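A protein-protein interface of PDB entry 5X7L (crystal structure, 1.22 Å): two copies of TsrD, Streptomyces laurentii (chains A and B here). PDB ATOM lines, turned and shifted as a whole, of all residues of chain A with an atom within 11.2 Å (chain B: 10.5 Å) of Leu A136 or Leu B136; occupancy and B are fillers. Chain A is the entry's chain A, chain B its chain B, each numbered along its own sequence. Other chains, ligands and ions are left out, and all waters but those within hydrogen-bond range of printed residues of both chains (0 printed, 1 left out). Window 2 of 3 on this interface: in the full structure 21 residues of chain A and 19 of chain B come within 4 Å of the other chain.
Of the 20 printed residues of chain B, 4 touch a printed residue of chain A.
Ile A95 touches none of the printed residues of chain B.
Of the printed residues of chain B, Leu A126 touches Leu B127 (3.8 Å).
Of chain B, only Leu B126 (3.7 Å), Leu B127 (3.9 Å) and His B130 (3.5 Å) come within 4 Å of Leu A127.
His A130 touches just one residue of chain B: Leu B127.
Of the printed residues of chain B, Arg A131 touches His B130 (3.8 Å).
No residue of chain B comes within 4 Å of Ala A135.
Of chain B, only Leu B136 (3.5 Å) comes within 4 Å of Leu A136.
Arg B100 touches none of the printed residues of chain A.
Of the printed residues of chain A, Leu B126 touches Leu A127.
Of the printed residues of chain A, Leu B127 touches Leu A126, Leu A127 and His A130.
Printed residues of chain A within 4 Å of His B130: Leu A127 (3.5 Å) and Arg A131 (3.8 Å).
No residue of chain A comes within 4 Å of Gly B134.
No residue of chain A comes within 4 Å of Ala B135.
Of chain A, only Leu A136 (3.5 Å) comes within 4 Å of Leu B136.
No residue of chain A comes within 4 Å of Pro B137.
The nearest residue of chain A that does not touch Leu B136 is Leu A127 (4.2 Å).
Leu A126 touches Leu B127, and with the chains exchanged Leu A127 touches Leu B126.
Leu A127 touches its own counterpart, Leu B127.
Leu A127 touches His B130, and with the chains exchanged His A130 touches Leu B127.
Leu B136 touches its own counterpart, Leu A136.
19 positions are printed for both chains.
N of Leu B136 lies within hydrogen-bond range of O of His B130, at 3.4 Å.
A ring nitrogen (ND1) of His B130 lies within hydrogen-bond range of the backbone carbonyl oxygen (O) of Leu B126 (2.9 Å).
O of His A130 is in hydrogen-bond range of N of Ala A135, at 2.9 Å.
O of His B130 is in hydrogen-bond range of N of Ala B135, 2.9 Å away.
The backbone carbonyl oxygen (O) of Leu A126 sits at hydrogen-bond distance from a ring nitrogen (ND1) of His A130 (2.8 Å).
Among the printed residues, merely in contact across the chains: Leu A136 with Leu B136, Leu A127 with His B130, Leu A127 with Leu B126, His A130 with Leu B127, Leu A126 with Leu B127, Arg A131 with His B130 and Leu A127 with Leu B127.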
ATOM      1  N   GLN A  88      26.681  26.995 -17.674  1.00  0.00           N
ATOM      2  CA  GLN A  88      26.463  27.291 -16.262  1.00  0.00           C
ATOM      3  C   GLN A  88      27.766  27.299 -15.475  1.00  0.00           C
ATOM      4  O   GLN A  88      28.429  26.272 -15.368  1.00  0.00           O
ATOM      5  CB  GLN A  88      25.521  26.278 -15.618  1.00  0.00           C
ATOM      6  CG  GLN A  88      25.351  26.562 -14.135  1.00  0.00           C
ATOM      7  CD  GLN A  88      24.526  25.536 -13.391  1.00  0.00           C
ATOM      8  OE1 GLN A  88      24.465  24.368 -13.775  1.00  0.00           O
ATOM      9  NE2 GLN A  88      23.901  25.966 -12.301  1.00  0.00           N
ATOM     10  N   ILE A  92      22.138  28.289 -10.527  1.00  0.00           N
ATOM     11  CA  ILE A  92      20.970  28.676 -11.309  1.00  0.00           C
ATOM     12  C   ILE A  92      19.751  27.975 -10.725  1.00  0.00           C
ATOM     13  O   ILE A  92      19.660  26.750 -10.771  1.00  0.00           O
ATOM     14  CB  ILE A  92      21.123  28.301 -12.798  1.00  0.00           C
ATOM     15  CG1 ILE A  92      22.264  29.101 -13.438  1.00  0.00           C
ATOM     16  CG2 ILE A  92      19.819  28.548 -13.547  1.00  0.00           C
ATOM     17  CD1 ILE A  92      22.559  28.723 -14.879  1.00  0.00           C
ATOM     18  N   LEU A  93      18.825  28.755 -10.171  1.00  0.00           N
ATOM     19  CA  LEU A  93      17.594  28.220  -9.586  1.00  0.00           C
ATOM     20  C   LEU A  93      17.859  27.101  -8.578  1.00  0.00           C
ATOM     21  O   LEU A  93      17.151  26.092  -8.550  1.00  0.00           O
ATOM     22  CB  LEU A  93      16.659  27.726 -10.692  1.00  0.00           C
ATOM     23  CG  LEU A  93      16.278  28.790 -11.721  1.00  0.00           C
ATOM     24  CD1 LEU A  93      15.554  28.161 -12.901  1.00  0.00           C
ATOM     25  CD2 LEU A  93      15.425  29.873 -11.076  1.00  0.00           C
ATOM     26  N   GLY A  94      18.889  27.284  -7.758  1.00  0.00           N
ATOM     27  CA  GLY A  94      19.228  26.319  -6.720  1.00  0.00           C
ATOM     28  C   GLY A  94      20.109  25.175  -7.192  1.00  0.00           C
ATOM     29  O   GLY A  94      20.567  24.370  -6.380  1.00  0.00           O
ATOM     30  N   ILE A  95      20.343  25.098  -8.499  1.00  0.00           N
ATOM     31  CA  ILE A  95      21.215  24.080  -9.071  1.00  0.00           C
ATOM     32  C   ILE A  95      22.661  24.543  -8.952  1.00  0.00           C
ATOM     33  O   ILE A  95      23.016  25.586  -9.501  1.00  0.00           O
ATOM     34  CB  ILE A  95      20.898  23.822 -10.559  1.00  0.00           C
ATOM     35  CG1 ILE A  95      19.419  23.468 -10.742  1.00  0.00           C
ATOM     36  CG2 ILE A  95      21.794  22.719 -11.113  1.00  0.00           C
ATOM     37  CD1 ILE A  95      18.952  23.516 -12.181  1.00  0.00           C
ATOM     38  N   PRO A  96      23.501  23.773  -8.238  1.00  0.00           N
ATOM     39  CA  PRO A  96      24.919  24.127  -8.143  1.00  0.00           C
ATOM     40  C   PRO A  96      25.592  24.194  -9.511  1.00  0.00           C
ATOM     41  O   PRO A  96      25.155  23.522 -10.447  1.00  0.00           O
ATOM     42  CB  PRO A  96      25.512  22.987  -7.306  1.00  0.00           C
ATOM     43  CG  PRO A  96      24.360  22.441  -6.536  1.00  0.00           C
ATOM     44  CD  PRO A  96      23.184  22.566  -7.453  1.00  0.00           C
ATOM     45  N   SER A  98      27.244  23.508 -12.628  1.00  0.00           N
ATOM     46  CA  SER A  98      27.511  22.214 -13.258  1.00  0.00           C
ATOM     47  C   SER A  98      28.596  22.271 -14.327  1.00  0.00           C
ATOM     48  O   SER A  98      29.172  21.247 -14.685  1.00  0.00           O
ATOM     49  CB  SER A  98      26.235  21.659 -13.891  1.00  0.00           C
ATOM     50  OG  SER A  98      25.860  22.426 -15.023  1.00  0.00           O
ATOM     51  N   ARG A 100      27.887  22.854 -17.310  1.00  0.00           N
ATOM     52  CA  ARG A 100      27.251  22.292 -18.499  1.00  0.00           C
ATOM     53  C   ARG A 100      26.625  23.356 -19.386  1.00  0.00           C
ATOM     54  O   ARG A 100      26.181  24.406 -18.912  1.00  0.00           O
ATOM     55  CB  ARG A 100      26.181  21.276 -18.105  1.00  0.00           C
ATOM     56  CG  ARG A 100      26.732  20.092 -17.329  1.00  0.00           C
ATOM     57  CD  ARG A 100      25.625  19.293 -16.665  1.00  0.00           C
ATOM     58  NE  ARG A 100      24.749  18.642 -17.635  1.00  0.00           N
ATOM     59  CZ  ARG A 100      24.842  17.364 -17.986  1.00  0.00           C
ATOM     60  N   ASP A 125      11.116  27.213 -20.817  1.00  0.00           N
ATOM     61  CA  ASP A 125      11.314  25.777 -20.664  1.00  0.00           C
ATOM     62  C   ASP A 125      12.259  25.473 -19.496  1.00  0.00           C
ATOM     63  O   ASP A 125      13.390  25.014 -19.682  1.00  0.00           O
ATOM     64  CB  ASP A 125      11.835  25.187 -21.977  1.00  0.00           C
ATOM     65  CG  ASP A 125      11.958  23.674 -21.943  1.00  0.00           C
ATOM     66  OD1 ASP A 125      11.359  23.023 -21.060  1.00  0.00           O
ATOM     67  OD2 ASP A 125      12.669  23.133 -22.812  1.00  0.00           O
ATOM     68  N   LEU A 126      11.773  25.730 -18.286  1.00  0.00           N
ATOM     69  CA  LEU A 126      12.548  25.490 -17.073  1.00  0.00           C
ATOM     70  C   LEU A 126      12.754  24.000 -16.816  1.00  0.00           C
ATOM     71  O   LEU A 126      13.774  23.608 -16.251  1.00  0.00           O
ATOM     72  CB  LEU A 126      11.878  26.156 -15.869  1.00  0.00           C
ATOM     73  CG  LEU A 126      11.790  27.685 -15.936  1.00  0.00           C
ATOM     74  CD1 LEU A 126      11.077  28.228 -14.707  1.00  0.00           C
ATOM     75  CD2 LEU A 126      13.166  28.323 -16.081  1.00  0.00           C
ATOM     76  N   LEU A 127      11.803  23.169 -17.240  1.00  0.00           N
ATOM     77  CA  LEU A 127      11.986  21.724 -17.149  1.00  0.00           C
ATOM     78  C   LEU A 127      13.205  21.308 -17.973  1.00  0.00           C
ATOM     79  O   LEU A 127      14.058  20.556 -17.501  1.00  0.00           O
ATOM     80  CB  LEU A 127      10.741  20.975 -17.627  1.00  0.00           C
ATOM     81  CG  LEU A 127      10.854  19.449 -17.546  1.00  0.00           C
ATOM     82  CD1 LEU A 127      11.027  18.984 -16.104  1.00  0.00           C
ATOM     83  CD2 LEU A 127       9.642  18.793 -18.186  1.00  0.00           C
ATOM     84  N   GLY A 128      13.279  21.806 -19.204  1.00  0.00           N
ATOM     85  CA  GLY A 128      14.421  21.548 -20.068  1.00  0.00           C
ATOM     86  C   GLY A 128      15.721  22.061 -19.479  1.00  0.00           C
ATOM     87  O   GLY A 128      16.752  21.400 -19.575  1.00  0.00           O
ATOM     88  N   LEU A 129      15.677  23.236 -18.859  1.00  0.00           N
ATOM     89  CA  LEU A 129      16.874  23.798 -18.242  1.00  0.00           C
ATOM     90  C   LEU A 129      17.382  22.894 -17.115  1.00  0.00           C
ATOM     91  O   LEU A 129      18.578  22.606 -17.028  1.00  0.00           O
ATOM     92  CB  LEU A 129      16.593  25.207 -17.720  1.00  0.00           C
ATOM     93  CG  LEU A 129      17.780  25.973 -17.134  1.00  0.00           C
ATOM     94  CD1 LEU A 129      18.890  26.146 -18.165  1.00  0.00           C
ATOM     95  CD2 LEU A 129      17.309  27.320 -16.605  1.00  0.00           C
ATOM     96  N   HIS A 130      16.467  22.437 -16.265  1.00  0.00           N
ATOM     97  CA  HIS A 130      16.824  21.508 -15.193  1.00  0.00           C
ATOM     98  C   HIS A 130      17.430  20.219 -15.748  1.00  0.00           C
ATOM     99  O   HIS A 130      18.426  19.723 -15.224  1.00  0.00           O
ATOM    100  CB  HIS A 130      15.604  21.177 -14.332  1.00  0.00           C
ATOM    101  CG  HIS A 130      15.295  22.208 -13.293  1.00  0.00           C
ATOM    102  ND1 HIS A 130      14.710  23.419 -13.595  1.00  0.00           N
ATOM    103  CD2 HIS A 130      15.477  22.202 -11.951  1.00  0.00           C
ATOM    104  CE1 HIS A 130      14.551  24.117 -12.485  1.00  0.00           C
ATOM    105  NE2 HIS A 130      15.008  23.401 -11.473  1.00  0.00           N
ATOM    106  N   ARG A 131      16.824  19.688 -16.805  1.00  0.00           N
ATOM    107  CA  ARG A 131      17.306  18.455 -17.430  1.00  0.00           C
ATOM    108  C   ARG A 131      18.701  18.632 -18.023  1.00  0.00           C
ATOM    109  O   ARG A 131      19.585  17.799 -17.817  1.00  0.00           O
ATOM    110  CB  ARG A 131      16.334  17.984 -18.516  1.00  0.00           C
ATOM    111  CG  ARG A 131      15.335  16.944 -18.039  1.00  0.00           C
ATOM    112  CD  ARG A 131      14.126  16.876 -18.954  1.00  0.00           C
ATOM    113  NE  ARG A 131      13.028  16.121 -18.354  1.00  0.00           N
ATOM    114  CZ  ARG A 131      11.839  15.941 -18.923  1.00  0.00           C
ATOM    115  NH1 ARG A 131      11.577  16.463 -20.116  1.00  0.00           N
ATOM    116  NH2 ARG A 131      10.905  15.236 -18.296  1.00  0.00           N
ATOM    117  N   GLN A 132      18.896  19.723 -18.753  1.00  0.00           N
ATOM    118  CA  GLN A 132      20.173  19.980 -19.410  1.00  0.00           C
ATOM    119  C   GLN A 132      21.298  20.199 -18.403  1.00  0.00           C
ATOM    120  O   GLN A 132      22.440  19.813 -18.656  1.00  0.00           O
ATOM    121  CB  GLN A 132      20.052  21.185 -20.342  1.00  0.00           C
ATOM    122  CG  GLN A 132      19.156  20.935 -21.543  1.00  0.00           C
ATOM    123  CD  GLN A 132      18.875  22.198 -22.328  1.00  0.00           C
ATOM    124  OE1 GLN A 132      19.499  23.230 -22.094  1.00  0.00           O
ATOM    125  NE2 GLN A 132      17.934  22.127 -23.263  1.00  0.00           N
ATOM    126  N   LEU A 133      20.977  20.799 -17.259  1.00  0.00           N
ATOM    127  CA  LEU A 133      21.980  21.066 -16.228  1.00  0.00           C
ATOM    128  C   LEU A 133      22.160  19.896 -15.257  1.00  0.00           C
ATOM    129  O   LEU A 133      22.908  20.004 -14.287  1.00  0.00           O
ATOM    130  CB  LEU A 133      21.634  22.349 -15.467  1.00  0.00           C
ATOM    131  CG  LEU A 133      21.595  23.613 -16.332  1.00  0.00           C
ATOM    132  CD1 LEU A 133      21.259  24.834 -15.487  1.00  0.00           C
ATOM    133  CD2 LEU A 133      22.911  23.816 -17.071  1.00  0.00           C
ATOM    134  N   GLY A 134      21.482  18.784 -15.530  1.00  0.00           N
ATOM    135  CA  GLY A 134      21.673  17.550 -14.774  1.00  0.00           C
ATOM    136  C   GLY A 134      20.952  17.493 -13.439  1.00  0.00           C
ATOM    137  O   GLY A 134      21.260  16.646 -12.600  1.00  0.00           O
ATOM    138  N   ALA A 135      19.982  18.380 -13.244  1.00  0.00           N
ATOM    139  CA  ALA A 135      19.258  18.463 -11.976  1.00  0.00           C
ATOM    140  C   ALA A 135      18.054  17.522 -11.918  1.00  0.00           C
ATOM    141  O   ALA A 135      17.530  17.260 -10.837  1.00  0.00           O
ATOM    142  CB  ALA A 135      18.814  19.892 -11.720  1.00  0.00           C
ATOM    143  N   LEU A 136      17.616  17.029 -13.074  1.00  0.00           N
ATOM    144  CA  LEU A 136      16.493  16.092 -13.141  1.00  0.00           C
ATOM    145  C   LEU A 136      16.733  15.023 -14.202  1.00  0.00           C
ATOM    146  O   LEU A 136      17.409  15.267 -15.203  1.00  0.00           O
ATOM    147  CB  LEU A 136      15.186  16.832 -13.440  1.00  0.00           C
ATOM    148  CG  LEU A 136      14.733  17.910 -12.452  1.00  0.00           C
ATOM    149  CD1 LEU A 136      13.544  18.668 -13.017  1.00  0.00           C
ATOM    150  CD2 LEU A 136      14.386  17.304 -11.097  1.00  0.00           C
ATOM    151  N   GLN B  88      -5.753  14.911 -13.587  1.00  0.00           N
ATOM    152  CA  GLN B  88      -5.029  13.864 -14.298  1.00  0.00           C
ATOM    153  C   GLN B  88      -5.549  12.478 -13.934  1.00  0.00           C
ATOM    154  O   GLN B  88      -5.466  12.072 -12.776  1.00  0.00           O
ATOM    155  CB  GLN B  88      -3.535  13.920 -13.995  1.00  0.00           C
ATOM    156  CG  GLN B  88      -2.781  12.804 -14.702  1.00  0.00           C
ATOM    157  CD  GLN B  88      -1.331  12.679 -14.285  1.00  0.00           C
ATOM    158  OE1 GLN B  88      -0.962  13.006 -13.153  1.00  0.00           O
ATOM    159  NE2 GLN B  88      -0.499  12.174 -15.194  1.00  0.00           N
ATOM    160  N   LEU B  93       2.595  13.089 -20.591  1.00  0.00           N
ATOM    161  CA  LEU B  93       3.979  13.451 -20.902  1.00  0.00           C
ATOM    162  C   LEU B  93       4.994  12.755 -19.992  1.00  0.00           C
ATOM    163  O   LEU B  93       5.917  13.385 -19.474  1.00  0.00           O
ATOM    164  CB  LEU B  93       4.153  14.972 -20.821  1.00  0.00           C
ATOM    165  CG  LEU B  93       3.191  15.790 -21.690  1.00  0.00           C
ATOM    166  CD1 LEU B  93       3.314  17.271 -21.371  1.00  0.00           C
ATOM    167  CD2 LEU B  93       3.430  15.537 -23.174  1.00  0.00           C
ATOM    168  N   GLY B  94       4.804  11.454 -19.791  1.00  0.00           N
ATOM    169  CA  GLY B  94       5.716  10.658 -18.979  1.00  0.00           C
ATOM    170  C   GLY B  94       5.395  10.618 -17.494  1.00  0.00           C
ATOM    171  O   GLY B  94       6.046   9.895 -16.741  1.00  0.00           O
ATOM    172  N   ILE B  95       4.396  11.391 -17.072  1.00  0.00           N
ATOM    173  CA  ILE B  95       3.973  11.431 -15.673  1.00  0.00           C
ATOM    174  C   ILE B  95       2.853  10.419 -15.447  1.00  0.00           C
ATOM    175  O   ILE B  95       1.790  10.541 -16.050  1.00  0.00           O
ATOM    176  CB  ILE B  95       3.456  12.831 -15.268  1.00  0.00           C
ATOM    177  CG1 ILE B  95       4.491  13.916 -15.588  1.00  0.00           C
ATOM    178  CG2 ILE B  95       3.082  12.853 -13.788  1.00  0.00           C
ATOM    179  CD1 ILE B  95       3.930  15.325 -15.540  1.00  0.00           C
ATOM    180  N   PRO B  96       3.079   9.421 -14.576  1.00  0.00           N
ATOM    181  CA  PRO B  96       2.013   8.457 -14.285  1.00  0.00           C
ATOM    182  C   PRO B  96       0.769   9.128 -13.693  1.00  0.00           C
ATOM    183  O   PRO B  96       0.873  10.179 -13.059  1.00  0.00           O
ATOM    184  CB  PRO B  96       2.660   7.511 -13.265  1.00  0.00           C
ATOM    185  CG  PRO B  96       4.127   7.648 -13.494  1.00  0.00           C
ATOM    186  CD  PRO B  96       4.332   9.083 -13.879  1.00  0.00           C
ATOM    187  N   SER B  98      -1.811  10.585 -11.535  1.00  0.00           N
ATOM    188  CA  SER B  98      -1.741  10.962 -10.121  1.00  0.00           C
ATOM    189  C   SER B  98      -3.106  11.135  -9.466  1.00  0.00           C
ATOM    190  O   SER B  98      -3.208  11.145  -8.238  1.00  0.00           O
ATOM    191  CB  SER B  98      -0.973  12.273  -9.969  1.00  0.00           C
ATOM    192  OG  SER B  98      -1.697  13.347 -10.550  1.00  0.00           O
ATOM    193  N   ARG B 100      -4.547  13.909  -9.523  1.00  0.00           N
ATOM    194  CA  ARG B 100      -4.478  15.261  -8.964  1.00  0.00           C
ATOM    195  C   ARG B 100      -4.930  16.349  -9.930  1.00  0.00           C
ATOM    196  O   ARG B 100      -4.834  16.198 -11.151  1.00  0.00           O
ATOM    197  CB  ARG B 100      -3.049  15.586  -8.526  1.00  0.00           C
ATOM    198  CG  ARG B 100      -2.511  14.736  -7.394  1.00  0.00           C
ATOM    199  CD  ARG B 100      -1.101  15.182  -7.044  1.00  0.00           C
ATOM    200  NE  ARG B 100      -0.489  14.363  -6.004  1.00  0.00           N
ATOM    201  CZ  ARG B 100       0.747  14.541  -5.547  1.00  0.00           C
ATOM    202  N   ASP B 125       4.333  25.572 -19.044  1.00  0.00           N
ATOM    203  CA  ASP B 125       4.974  25.394 -17.741  1.00  0.00           C
ATOM    204  C   ASP B 125       5.014  23.910 -17.345  1.00  0.00           C
ATOM    205  O   ASP B 125       4.295  23.471 -16.442  1.00  0.00           O
ATOM    206  CB  ASP B 125       4.235  26.225 -16.687  1.00  0.00           C
ATOM    207  CG  ASP B 125       4.884  26.171 -15.314  1.00  0.00           C
ATOM    208  OD1 ASP B 125       6.053  25.738 -15.207  1.00  0.00           O
ATOM    209  OD2 ASP B 125       4.211  26.566 -14.339  1.00  0.00           O
ATOM    210  N   LEU B 126       5.862  23.143 -18.028  1.00  0.00           N
ATOM    211  CA  LEU B 126       5.962  21.710 -17.762  1.00  0.00           C
ATOM    212  C   LEU B 126       6.594  21.418 -16.407  1.00  0.00           C
ATOM    213  O   LEU B 126       6.256  20.422 -15.773  1.00  0.00           O
ATOM    214  CB  LEU B 126       6.745  20.998 -18.867  1.00  0.00           C
ATOM    215  CG  LEU B 126       6.083  20.990 -20.247  1.00  0.00           C
ATOM    216  CD1 LEU B 126       6.904  20.149 -21.211  1.00  0.00           C
ATOM    217  CD2 LEU B 126       4.655  20.477 -20.182  1.00  0.00           C
ATOM    218  N   LEU B 127       7.505  22.276 -15.955  1.00  0.00           N
ATOM    219  CA  LEU B 127       8.075  22.109 -14.621  1.00  0.00           C
ATOM    220  C   LEU B 127       6.968  22.206 -13.571  1.00  0.00           C
ATOM    221  O   LEU B 127       6.897  21.388 -12.652  1.00  0.00           O
ATOM    222  CB  LEU B 127       9.166  23.149 -14.347  1.00  0.00           C
ATOM    223  CG  LEU B 127       9.868  23.023 -12.987  1.00  0.00           C
ATOM    224  CD1 LEU B 127      10.577  21.681 -12.838  1.00  0.00           C
ATOM    225  CD2 LEU B 127      10.848  24.167 -12.788  1.00  0.00           C
ATOM    226  N   GLY B 128       6.099  23.202 -13.724  1.00  0.00           N
ATOM    227  CA  GLY B 128       4.948  23.364 -12.845  1.00  0.00           C
ATOM    228  C   GLY B 128       4.003  22.179 -12.920  1.00  0.00           C
ATOM    229  O   GLY B 128       3.479  21.735 -11.903  1.00  0.00           O
ATOM    230  N   LEU B 129       3.784  21.664 -14.127  1.00  0.00           N
ATOM    231  CA  LEU B 129       2.935  20.490 -14.312  1.00  0.00           C
ATOM    232  C   LEU B 129       3.491  19.287 -13.544  1.00  0.00           C
ATOM    233  O   LEU B 129       2.754  18.596 -12.835  1.00  0.00           O
ATOM    234  CB  LEU B 129       2.796  20.156 -15.799  1.00  0.00           C
ATOM    235  CG  LEU B 129       1.795  19.055 -16.147  1.00  0.00           C
ATOM    236  CD1 LEU B 129       0.371  19.477 -15.806  1.00  0.00           C
ATOM    237  CD2 LEU B 129       1.917  18.680 -17.618  1.00  0.00           C
ATOM    238  N   HIS B 130       4.793  19.050 -13.680  1.00  0.00           N
ATOM    239  CA  HIS B 130       5.457  17.966 -12.954  1.00  0.00           C
ATOM    240  C   HIS B 130       5.330  18.122 -11.445  1.00  0.00           C
ATOM    241  O   HIS B 130       5.074  17.151 -10.733  1.00  0.00           O
ATOM    242  CB  HIS B 130       6.933  17.888 -13.338  1.00  0.00           C
ATOM    243  CG  HIS B 130       7.187  17.119 -14.595  1.00  0.00           C
ATOM    244  ND1 HIS B 130       6.834  17.589 -15.841  1.00  0.00           N
ATOM    245  CD2 HIS B 130       7.757  15.908 -14.796  1.00  0.00           C
ATOM    246  CE1 HIS B 130       7.180  16.701 -16.756  1.00  0.00           C
ATOM    247  NE2 HIS B 130       7.740  15.672 -16.148  1.00  0.00           N
ATOM    248  N   ARG B 131       5.511  19.346 -10.961  1.00  0.00           N
ATOM    249  CA  ARG B 131       5.408  19.610  -9.529  1.00  0.00           C
ATOM    250  C   ARG B 131       3.991  19.391  -9.009  1.00  0.00           C
ATOM    251  O   ARG B 131       3.799  18.770  -7.966  1.00  0.00           O
ATOM    252  CB  ARG B 131       5.894  21.022  -9.210  1.00  0.00           C
ATOM    253  CG  ARG B 131       7.408  21.088  -9.136  1.00  0.00           C
ATOM    254  CD  ARG B 131       7.932  22.501  -9.001  1.00  0.00           C
ATOM    255  NE  ARG B 131       9.391  22.509  -8.914  1.00  0.00           N
ATOM    256  CZ  ARG B 131      10.158  23.565  -9.163  1.00  0.00           C
ATOM    257  NH1 ARG B 131       9.617  24.724  -9.523  1.00  0.00           N
ATOM    258  NH2 ARG B 131      11.479  23.462  -9.055  1.00  0.00           N
ATOM    259  N   GLN B 132       3.002  19.882  -9.745  1.00  0.00           N
ATOM    260  CA  GLN B 132       1.612  19.740  -9.325  1.00  0.00           C
ATOM    261  C   GLN B 132       1.142  18.289  -9.351  1.00  0.00           C
ATOM    262  O   GLN B 132       0.337  17.879  -8.512  1.00  0.00           O
ATOM    263  CB  GLN B 132       0.707  20.590 -10.206  1.00  0.00           C
ATOM    264  CG  GLN B 132       0.924  22.077 -10.031  1.00  0.00           C
ATOM    265  CD  GLN B 132       0.179  22.878 -11.070  1.00  0.00           C
ATOM    266  OE1 GLN B 132      -0.886  22.477 -11.517  1.00  0.00           O
ATOM    267  NE2 GLN B 132       0.740  24.007 -11.473  1.00  0.00           N
ATOM    268  N   LEU B 133       1.644  17.511 -10.303  1.00  0.00           N
ATOM    269  CA  LEU B 133       1.202  16.127 -10.454  1.00  0.00           C
ATOM    270  C   LEU B 133       2.076  15.136  -9.683  1.00  0.00           C
ATOM    271  O   LEU B 133       1.932  13.922  -9.838  1.00  0.00           O
ATOM    272  CB  LEU B 133       1.125  15.762 -11.937  1.00  0.00           C
ATOM    273  CG  LEU B 133       0.101  16.588 -12.724  1.00  0.00           C
ATOM    274  CD1 LEU B 133       0.072  16.158 -14.184  1.00  0.00           C
ATOM    275  CD2 LEU B 133      -1.294  16.505 -12.110  1.00  0.00           C
ATOM    276  N   GLY B 134       2.960  15.662  -8.839  1.00  0.00           N
ATOM    277  CA  GLY B 134       3.705  14.850  -7.882  1.00  0.00           C
ATOM    278  C   GLY B 134       4.915  14.130  -8.441  1.00  0.00           C
ATOM    279  O   GLY B 134       5.449  13.223  -7.803  1.00  0.00           O
ATOM    280  N   ALA B 135       5.355  14.535  -9.629  1.00  0.00           N
ATOM    281  CA  ALA B 135       6.495  13.901 -10.288  1.00  0.00           C
ATOM    282  C   ALA B 135       7.823  14.517  -9.855  1.00  0.00           C
ATOM    283  O   ALA B 135       8.879  13.909 -10.031  1.00  0.00           O
ATOM    284  CB  ALA B 135       6.344  13.988 -11.797  1.00  0.00           C
ATOM    285  N   LEU B 136       7.759  15.722  -9.296  1.00  0.00           N
ATOM    286  CA  LEU B 136       8.942  16.431  -8.820  1.00  0.00           C
ATOM    287  C   LEU B 136       8.643  17.154  -7.513  1.00  0.00           C
ATOM    288  O   LEU B 136       7.533  17.657  -7.323  1.00  0.00           O
ATOM    289  CB  LEU B 136       9.421  17.444  -9.863  1.00  0.00           C
ATOM    290  CG  LEU B 136       9.897  16.905 -11.212  1.00  0.00           C
ATOM    291  CD1 LEU B 136      10.225  18.063 -12.135  1.00  0.00           C
ATOM    292  CD2 LEU B 136      11.105  16.000 -11.039  1.00  0.00           C
ATOM    293  N   PRO B 137       9.631  17.212  -6.607  1.00  0.00           N
ATOM    294  CA  PRO B 137       9.474  17.961  -5.358  1.00  0.00           C
ATOM    295  C   PRO B 137       9.466  19.475  -5.576  1.00  0.00           C
ATOM    296  O   PRO B 137       9.768  19.941  -6.676  1.00  0.00           O
ATOM    297  CB  PRO B 137      10.698  17.539  -4.538  1.00  0.00           C
ATOM    298  CG  PRO B 137      11.707  17.120  -5.548  1.00  0.00           C
ATOM    299  CD  PRO B 137      10.926  16.510  -6.673  1.00  0.00           C
